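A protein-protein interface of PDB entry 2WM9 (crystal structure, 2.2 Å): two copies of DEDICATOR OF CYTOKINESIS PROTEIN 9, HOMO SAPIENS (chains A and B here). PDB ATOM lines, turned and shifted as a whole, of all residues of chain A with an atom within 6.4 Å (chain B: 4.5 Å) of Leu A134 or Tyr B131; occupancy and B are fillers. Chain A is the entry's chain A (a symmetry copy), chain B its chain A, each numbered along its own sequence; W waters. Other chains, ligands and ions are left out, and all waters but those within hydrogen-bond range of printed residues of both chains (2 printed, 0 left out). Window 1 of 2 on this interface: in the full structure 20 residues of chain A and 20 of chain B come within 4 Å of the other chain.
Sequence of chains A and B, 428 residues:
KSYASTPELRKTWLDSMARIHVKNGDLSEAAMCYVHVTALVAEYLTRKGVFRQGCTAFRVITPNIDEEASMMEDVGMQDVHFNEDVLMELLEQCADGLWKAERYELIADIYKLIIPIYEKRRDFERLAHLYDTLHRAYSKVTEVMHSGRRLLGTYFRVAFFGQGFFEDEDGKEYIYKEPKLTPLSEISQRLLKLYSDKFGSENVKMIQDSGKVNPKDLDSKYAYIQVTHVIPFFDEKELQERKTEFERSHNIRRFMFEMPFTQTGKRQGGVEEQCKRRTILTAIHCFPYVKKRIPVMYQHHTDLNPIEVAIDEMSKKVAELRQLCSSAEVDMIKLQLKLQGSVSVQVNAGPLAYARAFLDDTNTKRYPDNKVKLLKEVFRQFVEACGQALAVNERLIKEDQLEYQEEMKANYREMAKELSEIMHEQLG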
ATOM      1  N   TYR A 104      18.576 -12.870 -20.376  1.00  0.00           N
ATOM      2  CA  TYR A 104      17.329 -12.088 -20.465  1.00  0.00           C
ATOM      3  C   TYR A 104      17.134 -11.151 -19.287  1.00  0.00           C
ATOM      4  O   TYR A 104      16.769  -9.997 -19.465  1.00  0.00           O
ATOM      5  CB  TYR A 104      16.122 -13.021 -20.552  1.00  0.00           C
ATOM      6  CG  TYR A 104      16.297 -14.074 -21.594  1.00  0.00           C
ATOM      7  CD1 TYR A 104      16.271 -13.746 -22.956  1.00  0.00           C
ATOM      8  CD2 TYR A 104      16.500 -15.403 -21.231  1.00  0.00           C
ATOM      9  CE1 TYR A 104      16.430 -14.724 -23.931  1.00  0.00           C
ATOM     10  CE2 TYR A 104      16.675 -16.383 -22.198  1.00  0.00           C
ATOM     11  CZ  TYR A 104      16.633 -16.043 -23.536  1.00  0.00           C
ATOM     12  OH  TYR A 104      16.811 -17.024 -24.464  1.00  0.00           O
ATOM     13  N   ILE A 107      18.273  -7.367 -19.636  1.00  0.00           N
ATOM     14  CA  ILE A 107      17.835  -6.449 -20.681  1.00  0.00           C
ATOM     15  C   ILE A 107      17.212  -5.148 -20.109  1.00  0.00           C
ATOM     16  O   ILE A 107      17.505  -4.062 -20.619  1.00  0.00           O
ATOM     17  CB  ILE A 107      16.944  -7.168 -21.734  1.00  0.00           C
ATOM     18  CG1 ILE A 107      17.757  -8.323 -22.390  1.00  0.00           C
ATOM     19  CG2 ILE A 107      16.439  -6.168 -22.779  1.00  0.00           C
ATOM     20  CD1 ILE A 107      16.953  -9.247 -23.307  1.00  0.00           C
ATOM     21  N   ALA A 108      16.398  -5.255 -19.053  1.00  0.00           N
ATOM     22  CA  ALA A 108      15.743  -4.064 -18.471  1.00  0.00           C
ATOM     23  C   ALA A 108      16.757  -3.045 -17.959  1.00  0.00           C
ATOM     24  O   ALA A 108      16.555  -1.840 -18.105  1.00  0.00           O
ATOM     25  CB  ALA A 108      14.758  -4.432 -17.371  1.00  0.00           C
ATOM     26  N   ASP A 109      17.866  -3.520 -17.397  1.00  0.00           N
ATOM     27  CA  ASP A 109      18.913  -2.605 -16.951  1.00  0.00           C
ATOM     28  C   ASP A 109      19.397  -1.717 -18.109  1.00  0.00           C
ATOM     29  O   ASP A 109      19.686  -0.546 -17.914  1.00  0.00           O
ATOM     30  CB  ASP A 109      20.107  -3.363 -16.326  1.00  0.00           C
ATOM     31  CG  ASP A 109      19.750  -4.029 -14.981  1.00  0.00           C
ATOM     32  OD1 ASP A 109      19.045  -3.377 -14.165  1.00  0.00           O
ATOM     33  OD2 ASP A 109      20.174  -5.201 -14.742  1.00  0.00           O
ATOM     34  N   TYR A 111      17.469  -1.107 -20.882  1.00  0.00           N
ATOM     35  CA  TYR A 111      16.370  -0.300 -21.429  1.00  0.00           C
ATOM     36  C   TYR A 111      15.924   0.858 -20.518  1.00  0.00           C
ATOM     37  O   TYR A 111      15.498   1.908 -21.006  1.00  0.00           O
ATOM     38  CB  TYR A 111      15.208  -1.178 -21.880  1.00  0.00           C
ATOM     39  CG  TYR A 111      15.338  -1.692 -23.304  1.00  0.00           C
ATOM     40  CD1 TYR A 111      15.792  -0.853 -24.314  1.00  0.00           C
ATOM     41  CD2 TYR A 111      14.965  -3.007 -23.651  1.00  0.00           C
ATOM     42  CE1 TYR A 111      15.885  -1.281 -25.626  1.00  0.00           C
ATOM     43  CE2 TYR A 111      15.047  -3.457 -24.989  1.00  0.00           C
ATOM     44  CZ  TYR A 111      15.507  -2.578 -25.971  1.00  0.00           C
ATOM     45  OH  TYR A 111      15.590  -2.952 -27.304  1.00  0.00           O
ATOM     46  N   LYS A 112      16.075   0.694 -19.208  1.00  0.00           N
ATOM     47  CA  LYS A 112      15.830   1.817 -18.301  1.00  0.00           C
ATOM     48  C   LYS A 112      16.609   3.069 -18.712  1.00  0.00           C
ATOM     49  O   LYS A 112      16.174   4.183 -18.427  1.00  0.00           O
ATOM     50  CB  LYS A 112      16.159   1.452 -16.842  1.00  0.00           C
ATOM     51  CG  LYS A 112      15.229   0.374 -16.230  1.00  0.00           C
ATOM     52  CD  LYS A 112      15.879  -0.239 -14.935  1.00  0.00           C
ATOM     53  CE  LYS A 112      15.248  -1.577 -14.481  1.00  0.00           C
ATOM     54  NZ  LYS A 112      13.764  -1.590 -14.496  1.00  0.00           N
ATOM     55  N   ILE A 115      14.616   4.451 -22.168  1.00  0.00           N
ATOM     56  CA  ILE A 115      13.192   4.749 -22.063  1.00  0.00           C
ATOM     57  C   ILE A 115      12.823   6.266 -21.974  1.00  0.00           C
ATOM     58  O   ILE A 115      11.976   6.733 -22.743  1.00  0.00           O
ATOM     59  CB  ILE A 115      12.535   3.921 -20.911  1.00  0.00           C
ATOM     60  CG1 ILE A 115      12.392   2.458 -21.345  1.00  0.00           C
ATOM     61  CG2 ILE A 115      11.167   4.550 -20.485  1.00  0.00           C
ATOM     62  CD1 ILE A 115      12.123   1.451 -20.161  1.00  0.00           C
ATOM     63  N   HIS A 129       8.500  -1.252 -29.268  1.00  0.00           N
ATOM     64  CA  HIS A 129       9.443  -2.299 -29.594  1.00  0.00           C
ATOM     65  C   HIS A 129      10.211  -2.829 -28.363  1.00  0.00           C
ATOM     66  O   HIS A 129      10.336  -4.046 -28.172  1.00  0.00           O
ATOM     67  CB  HIS A 129      10.443  -1.854 -30.689  1.00  0.00           C
ATOM     68  CG  HIS A 129      11.506  -2.870 -30.925  1.00  0.00           C
ATOM     69  ND1 HIS A 129      12.794  -2.729 -30.445  1.00  0.00           N
ATOM     70  CD2 HIS A 129      11.434  -4.116 -31.455  1.00  0.00           C
ATOM     71  CE1 HIS A 129      13.491  -3.810 -30.745  1.00  0.00           C
ATOM     72  NE2 HIS A 129      12.689  -4.668 -31.356  1.00  0.00           N
ATOM     73  N   LEU A 130      10.730  -1.921 -27.542  1.00  0.00           N
ATOM     74  CA  LEU A 130      11.488  -2.341 -26.363  1.00  0.00           C
ATOM     75  C   LEU A 130      10.651  -3.045 -25.304  1.00  0.00           C
ATOM     76  O   LEU A 130      11.102  -4.021 -24.696  1.00  0.00           O
ATOM     77  CB  LEU A 130      12.371  -1.224 -25.786  1.00  0.00           C
ATOM     78  CG  LEU A 130      12.241  -0.146 -24.689  1.00  0.00           C
ATOM     79  CD1 LEU A 130      12.090   1.229 -25.301  1.00  0.00           C
ATOM     80  CD2 LEU A 130      11.251  -0.411 -23.514  1.00  0.00           C
ATOM     81  N   TYR A 131       9.414  -2.597 -25.135  1.00  0.00           N
ATOM     82  CA  TYR A 131       8.498  -3.289 -24.231  1.00  0.00           C
ATOM     83  C   TYR A 131       8.125  -4.686 -24.735  1.00  0.00           C
ATOM     84  O   TYR A 131       7.948  -5.612 -23.948  1.00  0.00           O
ATOM     85  CB  TYR A 131       7.251  -2.427 -23.987  1.00  0.00           C
ATOM     86  CG  TYR A 131       7.553  -1.218 -23.106  1.00  0.00           C
ATOM     87  CD1 TYR A 131       8.199  -1.379 -21.869  1.00  0.00           C
ATOM     88  CD2 TYR A 131       7.207   0.062 -23.506  1.00  0.00           C
ATOM     89  CE1 TYR A 131       8.482  -0.295 -21.053  1.00  0.00           C
ATOM     90  CE2 TYR A 131       7.484   1.188 -22.685  1.00  0.00           C
ATOM     91  CZ  TYR A 131       8.110   0.999 -21.459  1.00  0.00           C
ATOM     92  OH  TYR A 131       8.396   2.091 -20.667  1.00  0.00           O
ATOM     93  N   ASP A 132       8.012  -4.842 -26.050  1.00  0.00           N
ATOM     94  CA  ASP A 132       7.762  -6.156 -26.619  1.00  0.00           C
ATOM     95  C   ASP A 132       8.985  -7.064 -26.294  1.00  0.00           C
ATOM     96  O   ASP A 132       8.830  -8.181 -25.842  1.00  0.00           O
ATOM     97  CB  ASP A 132       7.509  -6.050 -28.123  1.00  0.00           C
ATOM     98  CG  ASP A 132       7.438  -7.420 -28.812  1.00  0.00           C
ATOM     99  OD1 ASP A 132       6.662  -8.268 -28.361  1.00  0.00           O
ATOM    100  OD2 ASP A 132       8.164  -7.661 -29.806  1.00  0.00           O
ATOM    101  N   THR A 133      10.184  -6.561 -26.507  1.00  0.00           N
ATOM    102  CA  THR A 133      11.366  -7.321 -26.113  1.00  0.00           C
ATOM    103  C   THR A 133      11.331  -7.669 -24.617  1.00  0.00           C
ATOM    104  O   THR A 133      11.607  -8.805 -24.250  1.00  0.00           O
ATOM    105  CB  THR A 133      12.706  -6.608 -26.465  1.00  0.00           C
ATOM    106  OG1 THR A 133      12.874  -6.552 -27.881  1.00  0.00           O
ATOM    107  CG2 THR A 133      13.877  -7.415 -25.899  1.00  0.00           C
ATOM    108  N   LEU A 134      10.979  -6.710 -23.755  1.00  0.00           N
ATOM    109  CA  LEU A 134      11.011  -7.000 -22.320  1.00  0.00           C
ATOM    110  C   LEU A 134      10.001  -8.073 -21.963  1.00  0.00           C
ATOM    111  O   LEU A 134      10.292  -8.989 -21.185  1.00  0.00           O
ATOM    112  CB  LEU A 134      10.817  -5.737 -21.472  1.00  0.00           C
ATOM    113  CG  LEU A 134      12.038  -4.804 -21.443  1.00  0.00           C
ATOM    114  CD1 LEU A 134      11.714  -3.544 -20.652  1.00  0.00           C
ATOM    115  CD2 LEU A 134      13.298  -5.508 -20.884  1.00  0.00           C
ATOM    116  N   HIS A 135       8.815  -7.979 -22.556  1.00  0.00           N
ATOM    117  CA  HIS A 135       7.801  -8.982 -22.316  1.00  0.00           C
ATOM    118  C   HIS A 135       8.295 -10.379 -22.717  1.00  0.00           C
ATOM    119  O   HIS A 135       8.145 -11.323 -21.963  1.00  0.00           O
ATOM    120  CB  HIS A 135       6.519  -8.671 -23.079  1.00  0.00           C
ATOM    121  CG  HIS A 135       5.583  -9.832 -23.149  1.00  0.00           C
ATOM    122  ND1 HIS A 135       5.133 -10.493 -22.021  1.00  0.00           N
ATOM    123  CD2 HIS A 135       5.012 -10.454 -24.203  1.00  0.00           C
ATOM    124  CE1 HIS A 135       4.335 -11.483 -22.383  1.00  0.00           C
ATOM    125  NE2 HIS A 135       4.225 -11.464 -23.699  1.00  0.00           N
ATOM    126  N   ARG A 136       8.862 -10.494 -23.908  1.00  0.00           N
ATOM    127  CA  ARG A 136       9.408 -11.753 -24.377  1.00  0.00           C
ATOM    128  C   ARG A 136      10.556 -12.210 -23.481  1.00  0.00           C
ATOM    129  O   ARG A 136      10.660 -13.375 -23.187  1.00  0.00           O
ATOM    130  CB  ARG A 136       9.911 -11.631 -25.815  1.00  0.00           C
ATOM    131  CG  ARG A 136       8.819 -11.510 -26.885  1.00  0.00           C
ATOM    132  CD  ARG A 136       9.464 -11.230 -28.252  1.00  0.00           C
ATOM    133  NE  ARG A 136       8.438 -10.939 -29.239  1.00  0.00           N
ATOM    134  CZ  ARG A 136       7.775 -11.869 -29.926  1.00  0.00           C
ATOM    135  NH1 ARG A 136       8.029 -13.163 -29.743  1.00  0.00           N
ATOM    136  NH2 ARG A 136       6.851 -11.506 -30.808  1.00  0.00           N
ATOM    137  N   ALA A 137      11.398 -11.283 -23.039  1.00  0.00           N
ATOM    138  CA  ALA A 137      12.496 -11.629 -22.161  1.00  0.00           C
ATOM    139  C   ALA A 137      12.001 -12.302 -20.858  1.00  0.00           C
ATOM    140  O   ALA A 137      12.456 -13.405 -20.506  1.00  0.00           O
ATOM    141  CB  ALA A 137      13.387 -10.394 -21.880  1.00  0.00           C
ATOM    142  N   TYR A 138      11.064 -11.655 -20.160  1.00  0.00           N
ATOM    143  CA  TYR A 138      10.503 -12.236 -18.937  1.00  0.00           C
ATOM    144  C   TYR A 138       9.700 -13.512 -19.182  1.00  0.00           C
ATOM    145  O   TYR A 138       9.705 -14.418 -18.338  1.00  0.00           O
ATOM    146  CB  TYR A 138       9.755 -11.193 -18.074  1.00  0.00           C
ATOM    147  CG  TYR A 138      10.765 -10.249 -17.484  1.00  0.00           C
ATOM    148  CD1 TYR A 138      11.553 -10.643 -16.402  1.00  0.00           C
ATOM    149  CD2 TYR A 138      11.000  -8.991 -18.060  1.00  0.00           C
ATOM    150  CE1 TYR A 138      12.497  -9.811 -15.878  1.00  0.00           C
ATOM    151  CE2 TYR A 138      11.944  -8.164 -17.568  1.00  0.00           C
ATOM    152  CZ  TYR A 138      12.692  -8.567 -16.464  1.00  0.00           C
ATOM    153  OH  TYR A 138      13.653  -7.722 -15.961  1.00  0.00           O
ATOM    154  N   SER A 139       9.048 -13.617 -20.340  1.00  0.00           N
ATOM    155  CA  SER A 139       8.468 -14.915 -20.713  1.00  0.00           C
ATOM    156  C   SER A 139       9.533 -16.012 -20.865  1.00  0.00           C
ATOM    157  O   SER A 139       9.310 -17.141 -20.427  1.00  0.00           O
ATOM    158  CB  SER A 139       7.682 -14.835 -22.017  1.00  0.00           C
ATOM    159  OG  SER A 139       6.519 -14.083 -21.833  1.00  0.00           O
ATOM    160  N   ILE B 115       7.627  -1.834 -10.886  1.00  0.00           N
ATOM    161  CA  ILE B 115       8.692  -2.626 -11.489  1.00  0.00           C
ATOM    162  C   ILE B 115       9.825  -3.088 -10.517  1.00  0.00           C
ATOM    163  O   ILE B 115      10.147  -4.280 -10.477  1.00  0.00           O
ATOM    164  CB  ILE B 115       9.266  -1.914 -12.757  1.00  0.00           C
ATOM    165  CG1 ILE B 115       8.265  -2.029 -13.911  1.00  0.00           C
ATOM    166  CG2 ILE B 115      10.672  -2.490 -13.130  1.00  0.00           C
ATOM    167  CD1 ILE B 115       8.527  -1.031 -15.103  1.00  0.00           C
ATOM    168  N   LEU B 127       6.319  -9.261 -14.038  1.00  0.00           N
ATOM    169  CA  LEU B 127       7.076  -8.395 -14.917  1.00  0.00           C
ATOM    170  C   LEU B 127       6.636  -8.681 -16.357  1.00  0.00           C
ATOM    171  O   LEU B 127       6.353  -7.751 -17.111  1.00  0.00           O
ATOM    172  CB  LEU B 127       8.598  -8.576 -14.707  1.00  0.00           C
ATOM    173  CG  LEU B 127       9.075  -7.898 -13.414  1.00  0.00           C
ATOM    174  CD1 LEU B 127      10.438  -8.397 -12.926  1.00  0.00           C
ATOM    175  CD2 LEU B 127       9.085  -6.370 -13.548  1.00  0.00           C
ATOM    176  N   ALA B 128       6.578  -9.963 -16.748  1.00  0.00           N
ATOM    177  CA  ALA B 128       6.164 -10.305 -18.107  1.00  0.00           C
ATOM    178  C   ALA B 128       4.795  -9.685 -18.444  1.00  0.00           C
ATOM    179  O   ALA B 128       4.581  -9.191 -19.549  1.00  0.00           O
ATOM    180  CB  ALA B 128       6.092 -11.853 -18.311  1.00  0.00           C
ATOM    181  N   HIS B 129       3.872  -9.750 -17.487  1.00  0.00           N
ATOM    182  CA  HIS B 129       2.534  -9.248 -17.709  1.00  0.00           C
ATOM    183  C   HIS B 129       2.489  -7.721 -17.937  1.00  0.00           C
ATOM    184  O   HIS B 129       1.830  -7.240 -18.869  1.00  0.00           O
ATOM    185  CB  HIS B 129       1.574  -9.639 -16.560  1.00  0.00           C
ATOM    186  CG  HIS B 129       0.235  -9.004 -16.707  1.00  0.00           C
ATOM    187  ND1 HIS B 129      -0.164  -7.917 -15.953  1.00  0.00           N
ATOM    188  CD2 HIS B 129      -0.740  -9.201 -17.629  1.00  0.00           C
ATOM    189  CE1 HIS B 129      -1.363  -7.528 -16.348  1.00  0.00           C
ATOM    190  NE2 HIS B 129      -1.734  -8.289 -17.366  1.00  0.00           N
ATOM    191  N   LEU B 130       3.175  -6.966 -17.085  1.00  0.00           N
ATOM    192  CA  LEU B 130       3.169  -5.508 -17.221  1.00  0.00           C
ATOM    193  C   LEU B 130       3.866  -4.998 -18.474  1.00  0.00           C
ATOM    194  O   LEU B 130       3.394  -4.052 -19.112  1.00  0.00           O
ATOM    195  CB  LEU B 130       3.621  -4.783 -15.944  1.00  0.00           C
ATOM    196  CG  LEU B 130       4.944  -4.216 -15.386  1.00  0.00           C
ATOM    197  CD1 LEU B 130       5.466  -5.079 -14.259  1.00  0.00           C
ATOM    198  CD2 LEU B 130       6.047  -3.793 -16.402  1.00  0.00           C
ATOM    199  N   TYR B 131       4.944  -5.666 -18.864  1.00  0.00           N
ATOM    200  CA  TYR B 131       5.605  -5.325 -20.122  1.00  0.00           C
ATOM    201  C   TYR B 131       4.735  -5.643 -21.343  1.00  0.00           C
ATOM    202  O   TYR B 131       4.762  -4.924 -22.338  1.00  0.00           O
ATOM    203  CB  TYR B 131       6.968  -6.026 -20.204  1.00  0.00           C
ATOM    204  CG  TYR B 131       7.987  -5.412 -19.250  1.00  0.00           C
ATOM    205  CD1 TYR B 131       8.228  -4.028 -19.257  1.00  0.00           C
ATOM    206  CD2 TYR B 131       8.692  -6.198 -18.353  1.00  0.00           C
ATOM    207  CE1 TYR B 131       9.151  -3.448 -18.400  1.00  0.00           C
ATOM    208  CE2 TYR B 131       9.645  -5.627 -17.468  1.00  0.00           C
ATOM    209  CZ  TYR B 131       9.875  -4.257 -17.505  1.00  0.00           C
ATOM    210  OH  TYR B 131      10.786  -3.696 -16.635  1.00  0.00           O
ATOM    211  N   ASP B 132       3.957  -6.717 -21.265  1.00  0.00           N
ATOM    212  CA  ASP B 132       3.026  -7.032 -22.336  1.00  0.00           C
ATOM    213  C   ASP B 132       1.977  -5.884 -22.418  1.00  0.00           C
ATOM    214  O   ASP B 132       1.690  -5.378 -23.485  1.00  0.00           O
ATOM    215  CB  ASP B 132       2.370  -8.392 -22.093  1.00  0.00           C
ATOM    216  CG  ASP B 132       1.233  -8.689 -23.080  1.00  0.00           C
ATOM    217  OD1 ASP B 132       1.463  -8.595 -24.290  1.00  0.00           O
ATOM    218  OD2 ASP B 132       0.099  -9.012 -22.653  1.00  0.00           O
ATOM    219  N   THR B 133       1.439  -5.474 -21.287  1.00  0.00           N
ATOM    220  CA  THR B 133       0.539  -4.325 -21.290  1.00  0.00           C
ATOM    221  C   THR B 133       1.221  -3.086 -21.890  1.00  0.00           C
ATOM    222  O   THR B 133       0.620  -2.397 -22.706  1.00  0.00           O
ATOM    223  CB  THR B 133      -0.041  -3.990 -19.884  1.00  0.00           C
ATOM    224  OG1 THR B 133      -0.921  -5.029 -19.456  1.00  0.00           O
ATOM    225  CG2 THR B 133      -0.863  -2.702 -19.966  1.00  0.00           C
ATOM    226  N   LEU B 134       2.470  -2.806 -21.506  1.00  0.00           N
ATOM    227  CA  LEU B 134       3.110  -1.589 -22.007  1.00  0.00           C
ATOM    228  C   LEU B 134       3.294  -1.656 -23.511  1.00  0.00           C
ATOM    229  O   LEU B 134       3.048  -0.678 -24.228  1.00  0.00           O
ATOM    230  CB  LEU B 134       4.433  -1.295 -21.289  1.00  0.00           C
ATOM    231  CG  LEU B 134       4.267  -0.772 -19.853  1.00  0.00           C
ATOM    232  CD1 LEU B 134       5.631  -0.597 -19.200  1.00  0.00           C
ATOM    233  CD2 LEU B 134       3.447   0.541 -19.801  1.00  0.00           C
ATOM    234  N   HIS B 135       3.702  -2.823 -23.998  1.00  0.00           N
ATOM    235  CA  HIS B 135       3.861  -2.999 -25.425  1.00  0.00           C
ATOM    236  C   HIS B 135       2.543  -2.740 -26.168  1.00  0.00           C
ATOM    237  O   HIS B 135       2.525  -2.027 -27.154  1.00  0.00           O
ATOM    238  CB  HIS B 135       4.352  -4.403 -25.760  1.00  0.00           C
ATOM    239  CG  HIS B 135       4.197  -4.748 -27.204  1.00  0.00           C
ATOM    240  ND1 HIS B 135       4.731  -3.970 -28.216  1.00  0.00           N
ATOM    241  CD2 HIS B 135       3.570  -5.777 -27.813  1.00  0.00           C
ATOM    242  CE1 HIS B 135       4.425  -4.504 -29.386  1.00  0.00           C
ATOM    243  NE2 HIS B 135       3.744  -5.614 -29.168  1.00  0.00           N
HETATM  244  O   HOH W   1      12.597  -1.243 -16.572  1.00  0.00           O
HETATM  245  O   HOH W   2      12.299  -5.271 -15.295  1.00  0.00           O
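Lys A112 touches Ile B115 (NZ to CG2, 3.5 Å). O of Tyr A131 touches O of Tyr B131 (3.6 Å). Tyr A131 touches Leu B134 (CE1 to CD1, 3.4 Å). CB of Tyr A131 touches N of His B135, at 3.6 Å. Asp A132 touches His B135 (CB to ND1, 3.5 Å). His A135 touches Tyr B131 (N to CB, 3.6 Å). His A135 touches Asp B132 (ND1 to CB, 3.5 Å). CD1 of Leu B127 touches CE1 of Tyr A138, at 3.9 Å. Tyr A138 touches Ala B128. Tyr A138 touches Tyr B131 (CE2 to CE2, 3.4 Å).
Tyr A131 touches its own counterpart, Tyr B131. Tyr A131 touches Leu B134, and with the chains exchanged Leu A134 touches Tyr B131. Tyr A131 touches His B135, and with the chains exchanged His A135 touches Tyr B131. Asp A132 touches His B135, and with the chains exchanged His A135 touches Asp B132. Positions printed for both chains: 115, 129, 130, 131, 132, 133, 134 and 135. Of the 13 pairs that touch across the chains among the printed residues, 7 have their exchanged pair printed and touching as well.
The side-chain carboxylate (OD1) of Asp A132 is in salt-bridge range of the guanidinium group (NE) of Arg A136 (3.3 Å). O of His A135 sits at hydrogen-bond distance from OG of Ser A139.
ND1 of His A135 sits at hydrogen-bond distance from O of Ala B128 (2.8 Å).
Printed residues of chain A that touch a printed residue of chain B: Lys A112, Tyr A131, Asp A132, Leu A134, His A135, Tyr A138 and Ser A139. Hydrophobic or aromatic side chains of chain A within 4 Å of the printed part of chain B: Tyr A131, Leu A134, His A135 and Tyr A138. Printed residues of chain B that touch a printed residue of chain A: Ile B115, Leu B127, Ala B128, Tyr B131, Asp B132, Leu B134 and His B135.
Water W1 bridges NZ of Lys A112 and OH of Tyr B131. Water W2 bridges OH of Tyr B131 (2.6 Å) and OH of Tyr A138 (2.9 Å).
Printed residues of chain B within 4 Å of Asp A132: His B135. Of chain B, only Tyr B131 (3.4 Å) comes within 4 Å of Leu A134. Of the printed residues of chain B, His A135 touches Ala B128, Tyr B131 and Asp B132. Printed residues of chain A within 4 Å of Tyr B131: Tyr A131 (3.6 Å), Leu A134 (3.4 Å), His A135 (3.6 Å) and Tyr A138 (3.4 Å).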
